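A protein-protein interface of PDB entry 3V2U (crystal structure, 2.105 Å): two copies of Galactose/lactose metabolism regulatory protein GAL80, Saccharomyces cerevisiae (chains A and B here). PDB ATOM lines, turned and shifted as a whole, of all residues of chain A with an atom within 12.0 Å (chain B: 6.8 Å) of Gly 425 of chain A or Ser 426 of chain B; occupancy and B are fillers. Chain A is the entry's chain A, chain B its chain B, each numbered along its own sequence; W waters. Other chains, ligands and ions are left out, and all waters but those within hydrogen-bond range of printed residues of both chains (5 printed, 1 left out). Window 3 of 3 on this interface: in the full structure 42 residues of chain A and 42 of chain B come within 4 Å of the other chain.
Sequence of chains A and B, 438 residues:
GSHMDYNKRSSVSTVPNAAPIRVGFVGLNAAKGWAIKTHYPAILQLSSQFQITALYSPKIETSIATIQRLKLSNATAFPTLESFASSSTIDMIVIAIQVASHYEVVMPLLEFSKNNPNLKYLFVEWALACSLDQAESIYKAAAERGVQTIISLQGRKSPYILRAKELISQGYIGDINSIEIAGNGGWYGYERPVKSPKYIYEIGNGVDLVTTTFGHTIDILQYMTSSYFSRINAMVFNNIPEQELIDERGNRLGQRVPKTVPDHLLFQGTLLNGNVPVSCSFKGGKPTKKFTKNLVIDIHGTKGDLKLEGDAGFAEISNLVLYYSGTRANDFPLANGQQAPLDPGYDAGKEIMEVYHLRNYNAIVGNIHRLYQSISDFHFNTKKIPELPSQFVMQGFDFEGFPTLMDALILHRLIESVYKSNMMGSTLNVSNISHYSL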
ATOM      1  N   ARG A 231      -8.951 -21.392  36.508  1.00  0.00           N
ATOM      2  CA  ARG A 231      -9.703 -21.274  35.259  1.00  0.00           C
ATOM      3  C   ARG A 231     -11.174 -21.029  35.561  1.00  0.00           C
ATOM      4  O   ARG A 231     -11.718 -21.561  36.522  1.00  0.00           O
ATOM      5  CB  ARG A 231      -9.518 -22.520  34.379  1.00  0.00           C
ATOM      6  CG  ARG A 231      -8.153 -22.545  33.690  1.00  0.00           C
ATOM      7  CD  ARG A 231      -7.774 -23.904  33.119  1.00  0.00           C
ATOM      8  NE  ARG A 231      -8.617 -24.345  32.006  1.00  0.00           N
ATOM      9  CZ  ARG A 231      -8.570 -23.842  30.773  1.00  0.00           C
ATOM     10  NH1 ARG A 231      -7.741 -22.840  30.483  1.00  0.00           N
ATOM     11  NH2 ARG A 231      -9.369 -24.333  29.828  1.00  0.00           N
ATOM     12  N   ILE A 232     -11.814 -20.204  34.743  1.00  0.00           N
ATOM     13  CA  ILE A 232     -13.226 -19.899  34.944  1.00  0.00           C
ATOM     14  C   ILE A 232     -14.012 -19.862  33.640  1.00  0.00           C
ATOM     15  O   ILE A 232     -13.466 -19.593  32.570  1.00  0.00           O
ATOM     16  CB  ILE A 232     -13.429 -18.559  35.696  1.00  0.00           C
ATOM     17  CG1 ILE A 232     -12.994 -17.373  34.836  1.00  0.00           C
ATOM     18  CG2 ILE A 232     -12.710 -18.576  37.056  1.00  0.00           C
ATOM     19  CD1 ILE A 232     -14.147 -16.580  34.257  1.00  0.00           C
ATOM     20  N   ASN A 233     -15.302 -20.148  33.737  1.00  0.00           N
ATOM     21  CA  ASN A 233     -16.216 -19.906  32.638  1.00  0.00           C
ATOM     22  C   ASN A 233     -17.517 -19.367  33.202  1.00  0.00           C
ATOM     23  O   ASN A 233     -18.034 -19.889  34.195  1.00  0.00           O
ATOM     24  CB  ASN A 233     -16.479 -21.195  31.849  1.00  0.00           C
ATOM     25  CG  ASN A 233     -17.321 -20.956  30.595  1.00  0.00           C
ATOM     26  OD1 ASN A 233     -16.791 -20.881  29.487  1.00  0.00           O
ATOM     27  ND2 ASN A 233     -18.631 -20.842  30.769  1.00  0.00           N
ATOM     28  N   ALA A 234     -18.051 -18.326  32.575  1.00  0.00           N
ATOM     29  CA  ALA A 234     -19.293 -17.730  33.060  1.00  0.00           C
ATOM     30  C   ALA A 234     -20.291 -17.502  31.940  1.00  0.00           C
ATOM     31  O   ALA A 234     -19.918 -17.269  30.799  1.00  0.00           O
ATOM     32  CB  ALA A 234     -19.015 -16.409  33.774  1.00  0.00           C
ATOM     33  N   MET A 235     -21.570 -17.566  32.293  1.00  0.00           N
ATOM     34  CA  MET A 235     -22.633 -17.187  31.401  1.00  0.00           C
ATOM     35  C   MET A 235     -23.526 -16.203  32.163  1.00  0.00           C
ATOM     36  O   MET A 235     -23.998 -16.496  33.271  1.00  0.00           O
ATOM     37  CB  MET A 235     -23.432 -18.417  30.944  1.00  0.00           C
ATOM     38  CG  MET A 235     -22.597 -19.494  30.244  1.00  0.00           C
ATOM     39  SD  MET A 235     -23.580 -20.864  29.574  1.00  0.00           S
ATOM     40  CE  MET A 235     -22.298 -21.945  28.956  1.00  0.00           C
ATOM     41  N   VAL A 236     -23.760 -15.047  31.555  1.00  0.00           N
ATOM     42  CA  VAL A 236     -24.497 -13.969  32.196  1.00  0.00           C
ATOM     43  C   VAL A 236     -25.794 -13.754  31.421  1.00  0.00           C
ATOM     44  O   VAL A 236     -25.780 -13.718  30.193  1.00  0.00           O
ATOM     45  CB  VAL A 236     -23.668 -12.665  32.195  1.00  0.00           C
ATOM     46  CG1 VAL A 236     -24.500 -11.480  32.703  1.00  0.00           C
ATOM     47  CG2 VAL A 236     -22.383 -12.840  33.018  1.00  0.00           C
ATOM     48  N   PHE A 237     -26.908 -13.618  32.133  1.00  0.00           N
ATOM     49  CA  PHE A 237     -28.217 -13.553  31.480  1.00  0.00           C
ATOM     50  C   PHE A 237     -29.001 -12.281  31.737  1.00  0.00           C
ATOM     51  O   PHE A 237     -28.988 -11.732  32.839  1.00  0.00           O
ATOM     52  CB  PHE A 237     -29.100 -14.724  31.938  1.00  0.00           C
ATOM     53  CG  PHE A 237     -28.553 -16.057  31.586  1.00  0.00           C
ATOM     54  CD1 PHE A 237     -27.521 -16.614  32.326  1.00  0.00           C
ATOM     55  CD2 PHE A 237     -29.076 -16.767  30.513  1.00  0.00           C
ATOM     56  CE1 PHE A 237     -27.009 -17.858  31.996  1.00  0.00           C
ATOM     57  CE2 PHE A 237     -28.570 -18.016  30.181  1.00  0.00           C
ATOM     58  CZ  PHE A 237     -27.530 -18.562  30.927  1.00  0.00           C
ATOM     59  N   LEU A 266     -24.377 -17.968  35.702  1.00  0.00           N
ATOM     60  CA  LEU A 266     -23.758 -19.277  35.836  1.00  0.00           C
ATOM     61  C   LEU A 266     -22.257 -19.097  35.848  1.00  0.00           C
ATOM     62  O   LEU A 266     -21.681 -18.484  34.935  1.00  0.00           O
ATOM     63  CB  LEU A 266     -24.141 -20.193  34.674  1.00  0.00           C
ATOM     64  CG  LEU A 266     -25.647 -20.468  34.503  1.00  0.00           C
ATOM     65  CD1 LEU A 266     -25.939 -21.185  33.179  1.00  0.00           C
ATOM     66  CD2 LEU A 266     -26.153 -21.286  35.670  1.00  0.00           C
ATOM     67  N   GLN A 268     -18.583 -21.332  36.687  1.00  0.00           N
ATOM     68  CA  GLN A 268     -17.894 -22.528  37.117  1.00  0.00           C
ATOM     69  C   GLN A 268     -16.403 -22.296  36.933  1.00  0.00           C
ATOM     70  O   GLN A 268     -15.987 -21.545  36.051  1.00  0.00           O
ATOM     71  CB  GLN A 268     -18.410 -23.788  36.364  1.00  0.00           C
ATOM     72  CG  GLN A 268     -18.182 -23.773  34.859  1.00  0.00           C
ATOM     73  CD  GLN A 268     -18.940 -24.879  34.094  1.00  0.00           C
ATOM     74  OE1 GLN A 268     -18.640 -25.151  32.930  1.00  0.00           O
ATOM     75  NE2 GLN A 268     -19.917 -25.506  34.741  1.00  0.00           N
ATOM     76  N   GLU A 416     -14.191  -8.792  35.977  1.00  0.00           N
ATOM     77  CA  GLU A 416     -13.940  -8.472  34.575  1.00  0.00           C
ATOM     78  C   GLU A 416     -13.839  -9.737  33.714  1.00  0.00           C
ATOM     79  O   GLU A 416     -14.403  -9.799  32.629  1.00  0.00           O
ATOM     80  CB  GLU A 416     -12.654  -7.657  34.437  1.00  0.00           C
ATOM     81  CG  GLU A 416     -12.203  -7.432  32.991  1.00  0.00           C
ATOM     82  CD  GLU A 416     -13.192  -6.616  32.170  1.00  0.00           C
ATOM     83  OE1 GLU A 416     -14.164  -6.082  32.750  1.00  0.00           O
ATOM     84  OE2 GLU A 416     -13.001  -6.524  30.937  1.00  0.00           O
ATOM     85  N   SER A 417     -13.117 -10.740  34.201  1.00  0.00           N
ATOM     86  CA  SER A 417     -12.961 -11.987  33.455  1.00  0.00           C
ATOM     87  C   SER A 417     -14.273 -12.780  33.376  1.00  0.00           C
ATOM     88  O   SER A 417     -14.483 -13.546  32.448  1.00  0.00           O
ATOM     89  CB  SER A 417     -11.866 -12.856  34.073  1.00  0.00           C
ATOM     90  OG  SER A 417     -12.303 -13.428  35.293  1.00  0.00           O
ATOM     91  N   VAL A 418     -15.146 -12.607  34.364  1.00  0.00           N
ATOM     92  CA  VAL A 418     -16.462 -13.232  34.307  1.00  0.00           C
ATOM     93  C   VAL A 418     -17.230 -12.643  33.127  1.00  0.00           C
ATOM     94  O   VAL A 418     -17.761 -13.382  32.297  1.00  0.00           O
ATOM     95  CB  VAL A 418     -17.255 -13.019  35.601  1.00  0.00           C
ATOM     96  CG1 VAL A 418     -18.735 -13.374  35.392  1.00  0.00           C
ATOM     97  CG2 VAL A 418     -16.644 -13.853  36.724  1.00  0.00           C
ATOM     98  N   TYR A 419     -17.267 -11.314  33.046  1.00  0.00           N
ATOM     99  CA  TYR A 419     -17.878 -10.637  31.906  1.00  0.00           C
ATOM    100  C   TYR A 419     -17.179 -10.927  30.573  1.00  0.00           C
ATOM    101  O   TYR A 419     -17.840 -11.128  29.550  1.00  0.00           O
ATOM    102  CB  TYR A 419     -17.974  -9.123  32.143  1.00  0.00           C
ATOM    103  CG  TYR A 419     -19.147  -8.725  33.024  1.00  0.00           C
ATOM    104  CD1 TYR A 419     -18.954  -8.291  34.327  1.00  0.00           C
ATOM    105  CD2 TYR A 419     -20.450  -8.800  32.549  1.00  0.00           C
ATOM    106  CE1 TYR A 419     -20.027  -7.921  35.129  1.00  0.00           C
ATOM    107  CE2 TYR A 419     -21.533  -8.444  33.343  1.00  0.00           C
ATOM    108  CZ  TYR A 419     -21.319  -8.003  34.634  1.00  0.00           C
ATOM    109  OH  TYR A 419     -22.403  -7.627  35.426  1.00  0.00           O
ATOM    110  N   LYS A 420     -15.853 -10.942  30.567  1.00  0.00           N
ATOM    111  CA  LYS A 420     -15.153 -11.270  29.328  1.00  0.00           C
ATOM    112  C   LYS A 420     -15.477 -12.701  28.894  1.00  0.00           C
ATOM    113  O   LYS A 420     -15.709 -12.969  27.717  1.00  0.00           O
ATOM    114  CB  LYS A 420     -13.637 -11.105  29.476  1.00  0.00           C
ATOM    115  CG  LYS A 420     -12.894 -11.215  28.145  1.00  0.00           C
ATOM    116  CD  LYS A 420     -11.380 -11.289  28.324  1.00  0.00           C
ATOM    117  CE  LYS A 420     -10.881 -10.179  29.236  1.00  0.00           C
ATOM    118  NZ  LYS A 420     -11.388  -8.836  28.826  1.00  0.00           N
ATOM    119  N   SER A 421     -15.487 -13.621  29.855  1.00  0.00           N
ATOM    120  CA  SER A 421     -15.750 -15.028  29.556  1.00  0.00           C
ATOM    121  C   SER A 421     -17.120 -15.190  28.897  1.00  0.00           C
ATOM    122  O   SER A 421     -17.276 -15.913  27.906  1.00  0.00           O
ATOM    123  CB  SER A 421     -15.688 -15.845  30.839  1.00  0.00           C
ATOM    124  OG  SER A 421     -16.196 -17.142  30.647  1.00  0.00           O
ATOM    125  N   ASN A 422     -18.118 -14.520  29.453  1.00  0.00           N
ATOM    126  CA  ASN A 422     -19.433 -14.490  28.830  1.00  0.00           C
ATOM    127  C   ASN A 422     -19.377 -13.924  27.411  1.00  0.00           C
ATOM    128  O   ASN A 422     -19.964 -14.478  26.492  1.00  0.00           O
ATOM    129  CB  ASN A 422     -20.401 -13.682  29.681  1.00  0.00           C
ATOM    130  CG  ASN A 422     -21.793 -13.650  29.096  1.00  0.00           C
ATOM    131  OD1 ASN A 422     -22.526 -14.649  29.119  1.00  0.00           O
ATOM    132  ND2 ASN A 422     -22.174 -12.504  28.582  1.00  0.00           N
ATOM    133  N   MET A 423     -18.652 -12.826  27.232  1.00  0.00           N
ATOM    134  CA  MET A 423     -18.635 -12.141  25.938  1.00  0.00           C
ATOM    135  C   MET A 423     -17.924 -12.954  24.851  1.00  0.00           C
ATOM    136  O   MET A 423     -18.353 -12.979  23.694  1.00  0.00           O
ATOM    137  CB  MET A 423     -18.008 -10.746  26.078  1.00  0.00           C
ATOM    138  CG  MET A 423     -17.674 -10.074  24.730  1.00  0.00           C
ATOM    139  SD  MET A 423     -16.693  -8.558  24.893  1.00  0.00           S
ATOM    140  CE  MET A 423     -15.257  -9.157  25.784  1.00  0.00           C
ATOM    141  N   MET A 424     -16.842 -13.631  25.227  1.00  0.00           N
ATOM    142  CA  MET A 424     -16.029 -14.370  24.254  1.00  0.00           C
ATOM    143  C   MET A 424     -16.468 -15.828  24.098  1.00  0.00           C
ATOM    144  O   MET A 424     -15.986 -16.531  23.217  1.00  0.00           O
ATOM    145  CB  MET A 424     -14.551 -14.330  24.656  1.00  0.00           C
ATOM    146  CG  MET A 424     -13.948 -12.921  24.765  1.00  0.00           C
ATOM    147  SD  MET A 424     -14.121 -11.940  23.251  1.00  0.00           S
ATOM    148  CE  MET A 424     -13.033 -12.805  22.107  1.00  0.00           C
ATOM    149  N   GLY A 425     -17.375 -16.290  24.951  1.00  0.00           N
ATOM    150  CA  GLY A 425     -17.745 -17.691  24.925  1.00  0.00           C
ATOM    151  C   GLY A 425     -16.561 -18.601  25.209  1.00  0.00           C
ATOM    152  O   GLY A 425     -16.371 -19.627  24.553  1.00  0.00           O
ATOM    153  N   SER A 426     -15.749 -18.252  26.198  1.00  0.00           N
ATOM    154  CA  SER A 426     -14.570 -19.071  26.440  1.00  0.00           C
ATOM    155  C   SER A 426     -14.211 -19.191  27.905  1.00  0.00           C
ATOM    156  O   SER A 426     -14.535 -18.332  28.725  1.00  0.00           O
ATOM    157  CB  SER A 426     -13.367 -18.587  25.601  1.00  0.00           C
ATOM    158  OG  SER A 426     -12.756 -17.457  26.176  1.00  0.00           O
ATOM    159  N   THR A 427     -13.569 -20.304  28.221  1.00  0.00           N
ATOM    160  CA  THR A 427     -13.006 -20.544  29.538  1.00  0.00           C
ATOM    161  C   THR A 427     -11.691 -19.766  29.650  1.00  0.00           C
ATOM    162  O   THR A 427     -10.815 -19.904  28.804  1.00  0.00           O
ATOM    163  CB  THR A 427     -12.741 -22.027  29.667  1.00  0.00           C
ATOM    164  OG1 THR A 427     -13.993 -22.706  29.526  1.00  0.00           O
ATOM    165  CG2 THR A 427     -12.092 -22.370  31.020  1.00  0.00           C
ATOM    166  N   LEU A 428     -11.559 -18.932  30.674  1.00  0.00           N
ATOM    167  CA  LEU A 428     -10.385 -18.073  30.775  1.00  0.00           C
ATOM    168  C   LEU A 428      -9.428 -18.544  31.865  1.00  0.00           C
ATOM    169  O   LEU A 428      -9.856 -18.994  32.934  1.00  0.00           O
ATOM    170  CB  LEU A 428     -10.806 -16.617  31.034  1.00  0.00           C
ATOM    171  CG  LEU A 428     -11.643 -16.006  29.904  1.00  0.00           C
ATOM    172  CD1 LEU A 428     -12.070 -14.561  30.181  1.00  0.00           C
ATOM    173  CD2 LEU A 428     -10.880 -16.107  28.587  1.00  0.00           C
ATOM    174  N   ASN A 429      -8.137 -18.438  31.575  1.00  0.00           N
ATOM    175  CA  ASN A 429      -7.095 -18.611  32.578  1.00  0.00           C
ATOM    176  C   ASN A 429      -6.896 -17.319  33.380  1.00  0.00           C
ATOM    177  O   ASN A 429      -6.417 -16.326  32.845  1.00  0.00           O
ATOM    178  CB  ASN A 429      -5.775 -19.023  31.903  1.00  0.00           C
ATOM    179  CG  ASN A 429      -4.682 -19.332  32.913  1.00  0.00           C
ATOM    180  OD1 ASN A 429      -4.578 -18.678  33.950  1.00  0.00           O
ATOM    181  ND2 ASN A 429      -3.874 -20.343  32.622  1.00  0.00           N
ATOM    182  N   ARG B 231     -26.611 -23.631  24.234  1.00  0.00           N
ATOM    183  CA  ARG B 231     -25.178 -23.415  24.431  1.00  0.00           C
ATOM    184  C   ARG B 231     -24.739 -24.107  25.695  1.00  0.00           C
ATOM    185  O   ARG B 231     -25.476 -24.132  26.673  1.00  0.00           O
ATOM    186  CB  ARG B 231     -24.842 -21.920  24.523  1.00  0.00           C
ATOM    187  CG  ARG B 231     -25.151 -21.134  23.252  1.00  0.00           C
ATOM    188  CD  ARG B 231     -24.881 -19.627  23.458  1.00  0.00           C
ATOM    189  NE  ARG B 231     -23.461 -19.303  23.324  1.00  0.00           N
ATOM    190  CZ  ARG B 231     -22.736 -18.644  24.231  1.00  0.00           C
ATOM    191  NH1 ARG B 231     -23.284 -18.230  25.365  1.00  0.00           N
ATOM    192  NH2 ARG B 231     -21.451 -18.395  24.000  1.00  0.00           N
ATOM    193  N   ILE B 232     -23.539 -24.667  25.661  1.00  0.00           N
ATOM    194  CA  ILE B 232     -22.991 -25.388  26.799  1.00  0.00           C
ATOM    195  C   ILE B 232     -21.512 -25.079  27.034  1.00  0.00           C
ATOM    196  O   ILE B 232     -20.753 -24.738  26.105  1.00  0.00           O
ATOM    197  CB  ILE B 232     -23.152 -26.921  26.623  1.00  0.00           C
ATOM    198  CG1 ILE B 232     -22.276 -27.428  25.475  1.00  0.00           C
ATOM    199  CG2 ILE B 232     -24.606 -27.286  26.358  1.00  0.00           C
ATOM    200  CD1 ILE B 232     -21.109 -28.275  25.920  1.00  0.00           C
ATOM    201  N   ASN B 233     -21.100 -25.190  28.290  1.00  0.00           N
ATOM    202  CA  ASN B 233     -19.681 -25.258  28.579  1.00  0.00           C
ATOM    203  C   ASN B 233     -19.426 -26.315  29.620  1.00  0.00           C
ATOM    204  O   ASN B 233     -20.161 -26.408  30.605  1.00  0.00           O
ATOM    205  CB  ASN B 233     -19.108 -23.924  29.093  1.00  0.00           C
ATOM    206  CG  ASN B 233     -17.632 -24.061  29.476  1.00  0.00           C
ATOM    207  OD1 ASN B 233     -16.762 -24.084  28.611  1.00  0.00           O
ATOM    208  ND2 ASN B 233     -17.355 -24.210  30.759  1.00  0.00           N
ATOM    209  N   ALA B 234     -18.362 -27.084  29.435  1.00  0.00           N
ATOM    210  CA  ALA B 234     -18.038 -28.138  30.395  1.00  0.00           C
ATOM    211  C   ALA B 234     -16.570 -28.104  30.838  1.00  0.00           C
ATOM    212  O   ALA B 234     -15.672 -27.734  30.074  1.00  0.00           O
ATOM    213  CB  ALA B 234     -18.384 -29.515  29.805  1.00  0.00           C
ATOM    214  N   SER B 417     -19.906 -33.055  22.559  1.00  0.00           N
ATOM    215  CA  SER B 417     -19.751 -31.611  22.664  1.00  0.00           C
ATOM    216  C   SER B 417     -19.286 -31.196  24.060  1.00  0.00           C
ATOM    217  O   SER B 417     -18.599 -30.194  24.218  1.00  0.00           O
ATOM    218  CB  SER B 417     -21.069 -30.913  22.334  1.00  0.00           C
ATOM    219  OG  SER B 417     -22.050 -31.218  23.307  1.00  0.00           O
ATOM    220  N   LYS B 420     -15.639 -31.909  23.962  1.00  0.00           N
ATOM    221  CA  LYS B 420     -14.991 -30.950  23.072  1.00  0.00           C
ATOM    222  C   LYS B 420     -14.883 -29.592  23.765  1.00  0.00           C
ATOM    223  O   LYS B 420     -13.852 -28.910  23.686  1.00  0.00           O
ATOM    224  CB  LYS B 420     -15.785 -30.820  21.776  1.00  0.00           C
ATOM    225  CG  LYS B 420     -15.065 -30.088  20.657  1.00  0.00           C
ATOM    226  CD  LYS B 420     -15.885 -30.146  19.380  1.00  0.00           C
ATOM    227  CE  LYS B 420     -16.338 -31.575  19.096  1.00  0.00           C
ATOM    228  NZ  LYS B 420     -17.146 -31.688  17.849  1.00  0.00           N
ATOM    229  N   SER B 421     -15.960 -29.209  24.444  1.00  0.00           N
ATOM    230  CA  SER B 421     -16.006 -27.942  25.159  1.00  0.00           C
ATOM    231  C   SER B 421     -14.880 -27.892  26.183  1.00  0.00           C
ATOM    232  O   SER B 421     -14.207 -26.874  26.346  1.00  0.00           O
ATOM    233  CB  SER B 421     -17.357 -27.792  25.873  1.00  0.00           C
ATOM    234  OG  SER B 421     -17.318 -26.706  26.763  1.00  0.00           O
ATOM    235  N   ASN B 422     -14.688 -29.000  26.881  1.00  0.00           N
ATOM    236  CA  ASN B 422     -13.612 -29.094  27.850  1.00  0.00           C
ATOM    237  C   ASN B 422     -12.241 -28.981  27.204  1.00  0.00           C
ATOM    238  O   ASN B 422     -11.361 -28.259  27.685  1.00  0.00           O
ATOM    239  CB  ASN B 422     -13.686 -30.409  28.612  1.00  0.00           C
ATOM    240  CG  ASN B 422     -12.513 -30.584  29.533  1.00  0.00           C
ATOM    241  OD1 ASN B 422     -12.420 -29.904  30.558  1.00  0.00           O
ATOM    242  ND2 ASN B 422     -11.587 -31.463  29.161  1.00  0.00           N
ATOM    243  N   MET B 423     -12.069 -29.707  26.107  1.00  0.00           N
ATOM    244  CA  MET B 423     -10.796 -29.728  25.395  1.00  0.00           C
ATOM    245  C   MET B 423     -10.438 -28.366  24.812  1.00  0.00           C
ATOM    246  O   MET B 423      -9.293 -27.930  24.895  1.00  0.00           O
ATOM    247  CB  MET B 423     -10.821 -30.768  24.275  1.00  0.00           C
ATOM    248  CG  MET B 423      -9.571 -30.715  23.389  1.00  0.00           C
ATOM    249  SD  MET B 423      -9.863 -31.382  21.736  1.00  0.00           S
ATOM    250  CE  MET B 423      -8.655 -30.456  20.775  1.00  0.00           C
ATOM    251  N   MET B 424     -11.429 -27.699  24.229  1.00  0.00           N
ATOM    252  CA  MET B 424     -11.221 -26.425  23.545  1.00  0.00           C
ATOM    253  C   MET B 424     -11.238 -25.240  24.501  1.00  0.00           C
ATOM    254  O   MET B 424     -10.790 -24.150  24.156  1.00  0.00           O
ATOM    255  CB  MET B 424     -12.307 -26.220  22.486  1.00  0.00           C
ATOM    256  CG  MET B 424     -12.306 -27.276  21.400  1.00  0.00           C
ATOM    257  SD  MET B 424     -10.777 -27.244  20.453  1.00  0.00           S
ATOM    258  CE  MET B 424     -10.902 -25.635  19.673  1.00  0.00           C
ATOM    259  N   GLY B 425     -11.767 -25.451  25.700  1.00  0.00           N
ATOM    260  CA  GLY B 425     -11.941 -24.359  26.639  1.00  0.00           C
ATOM    261  C   GLY B 425     -12.936 -23.355  26.078  1.00  0.00           C
ATOM    262  O   GLY B 425     -12.718 -22.152  26.164  1.00  0.00           O
ATOM    263  N   SER B 426     -14.036 -23.850  25.508  1.00  0.00           N
ATOM    264  CA  SER B 426     -15.003 -22.987  24.825  1.00  0.00           C
ATOM    265  C   SER B 426     -16.450 -23.283  25.194  1.00  0.00           C
ATOM    266  O   SER B 426     -16.821 -24.429  25.448  1.00  0.00           O
ATOM    267  CB  SER B 426     -14.877 -23.146  23.303  1.00  0.00           C
ATOM    268  OG  SER B 426     -13.525 -23.121  22.897  1.00  0.00           O
ATOM    269  N   THR B 427     -17.268 -22.240  25.175  1.00  0.00           N
ATOM    270  CA  THR B 427     -18.716 -22.371  25.278  1.00  0.00           C
ATOM    271  C   THR B 427     -19.263 -22.658  23.883  1.00  0.00           C
ATOM    272  O   THR B 427     -19.191 -21.798  23.005  1.00  0.00           O
ATOM    273  CB  THR B 427     -19.309 -21.071  25.814  1.00  0.00           C
ATOM    274  OG1 THR B 427     -18.678 -20.753  27.066  1.00  0.00           O
ATOM    275  CG2 THR B 427     -20.812 -21.198  26.002  1.00  0.00           C
ATOM    276  N   LEU B 428     -19.791 -23.866  23.672  1.00  0.00           N
ATOM    277  CA  LEU B 428     -20.197 -24.296  22.336  1.00  0.00           C
ATOM    278  C   LEU B 428     -21.669 -24.057  22.051  1.00  0.00           C
ATOM    279  O   LEU B 428     -22.508 -24.161  22.937  1.00  0.00           O
ATOM    280  CB  LEU B 428     -19.889 -25.789  22.123  1.00  0.00           C
ATOM    281  CG  LEU B 428     -18.421 -26.200  22.261  1.00  0.00           C
ATOM    282  CD1 LEU B 428     -18.223 -27.729  22.133  1.00  0.00           C
ATOM    283  CD2 LEU B 428     -17.604 -25.455  21.218  1.00  0.00           C
HETATM  284  O   HOH W   1     -20.940 -17.103  26.770  1.00  0.00           O
HETATM  285  O   HOH W   2     -11.509 -26.314  29.766  1.00  0.00           O
HETATM  286  O   HOH W   3     -19.164 -18.390  28.377  1.00  0.00           O
HETATM  287  O   HOH W   4     -17.144 -20.556  21.662  1.00  0.00           O
HETATM  288  O   HOH W   5     -14.130 -25.287  29.680  1.00  0.00           O
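O of Ser 426 of chain A lies close to OD1 of Asn 233 of chain A (3.5 Å).
N of Leu 428 of chain B sits at hydrogen-bond distance from O of Ile 232 of chain B, 2.8 Å away.
The side-chain amide oxygen of Asn 233 of chain B sits close to the backbone carbonyl oxygen of Ser 426 of chain B, 3.2 Å away.
Asn 233 of chain A touches its own counterpart, Asn 233 of chain B.
Gly 425 of chain A touches Ser 426 of chain B, and with the chains exchanged Ser 426 of chain A touches Gly 425 of chain B.
14 positions are printed for both chains.
Of the 14 pairs that touch across the chains among the printed residues, 7 have their exchanged pair printed and touching as well.
The side-chain amide oxygen (OD1) of Asn 233 of chain A lies close to the side-chain amide oxygen (OD1) of Asn 233 of chain B, at 3.3 Å.
The side-chain amide oxygen of Asn 233 of chain A sits at hydrogen-bond distance from the side-chain hydroxyl of Thr 427 of chain B, 3.1 Å away.
The side-chain amide nitrogen (ND2) of Asn 233 of chain B lies within hydrogen-bond range of the side-chain amide oxygen (OE1) of Gln 268 of chain A.
The backbone carbonyl oxygen of Gly 425 of chain A lies within hydrogen-bond range of the backbone NH of Thr 427 of chain B (2.8 Å).
OG1 of Thr 427 of chain A is in hydrogen-bond range of OD1 of Asn 233 of chain B, at 3.2 Å.
N of Thr 427 of chain A is in hydrogen-bond range of O of Gly 425 of chain B.
Printed residues of chain B within 4 Å of Met 235 of chain A: Ile 232, Asn 233 and Thr 427.
Phe 237 of chain A touches none of the printed residues of chain B.
Gly 425 of chain A touches just these residues of chain B: Arg 231, Ser 426 and Thr 427.
Leu 428 of chain A touches none of the printed residues of chain B.
Of the printed residues of chain A, Ile 232 of chain B touches Met 235 (3.8 Å).
Ala 234 of chain B touches one residue of chain A.
No residue of chain A comes within 4 Å of Ser 421 of chain B.
Gly 425 of chain B touches just these residues of chain A: Ser 426 (3.6 Å) and Thr 427 (2.9 Å).
Of chain A, only Gly 425 comes within 4 Å of Ser 426 of chain B.
The nearest residue of chain B that does not touch Gly 425 of chain A is Gly 425 of chain B (4.7 Å).
The nearest residue of chain A that does not touch Ser 426 of chain B is Thr 427 of chain A (4.2 Å).
Water W5 lies within hydrogen-bond range of the side-chain hydroxyl (OG1) of Thr 427 of chain A, the backbone carbonyl oxygen (O) of Ala 234 of chain B and the side-chain amide oxygen (OD1) of Asn 233 of chain B.
Water W1 lies within hydrogen-bond range of O of Asn 422 of chain A (2.8 Å) and NH1 of Arg 231 of chain B (3.0 Å).
Among the printed residues, merely in contact across the chains: Met 235 of chain A with Ile 232 of chain B (3.8 Å), Met 235 of chain A with Asn 233 of chain B (3.5 Å), Met 235 of chain A with Thr 427 of chain B (3.4 Å), Gln 268 of chain A with Ala 234 of chain B (3.96 Å), Gly 425 of chain A with Arg 231 of chain B (3.9 Å), Gly 425 of chain A with Ser 426 of chain B (3.6 Å), Ser 426 of chain A with Gly 425 of chain B (3.6 Å) and Ser 426 of chain A with Thr 427 of chain B (3.9 Å).
Printed residues of chain A that touch a printed residue of chain B: Asn 233, Met 235, Gln 268, Gly 425, Ser 426 and Thr 427.
Hydrophobic or aromatic side chains of chain A within 4 Å of the printed part of chain B: Met 235.
Printed residues of chain B that touch a printed residue of chain A: Arg 231, Ile 232, Asn 233, Ala 234, Gly 425, Ser 426 and Thr 427.
Among the printed residues, 14 pairs touch across the chains.
Among the printed residues, no Asp or Glu carboxylate lies within 4 Å of a Lys or Arg side-chain nitrogen of the other chain.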
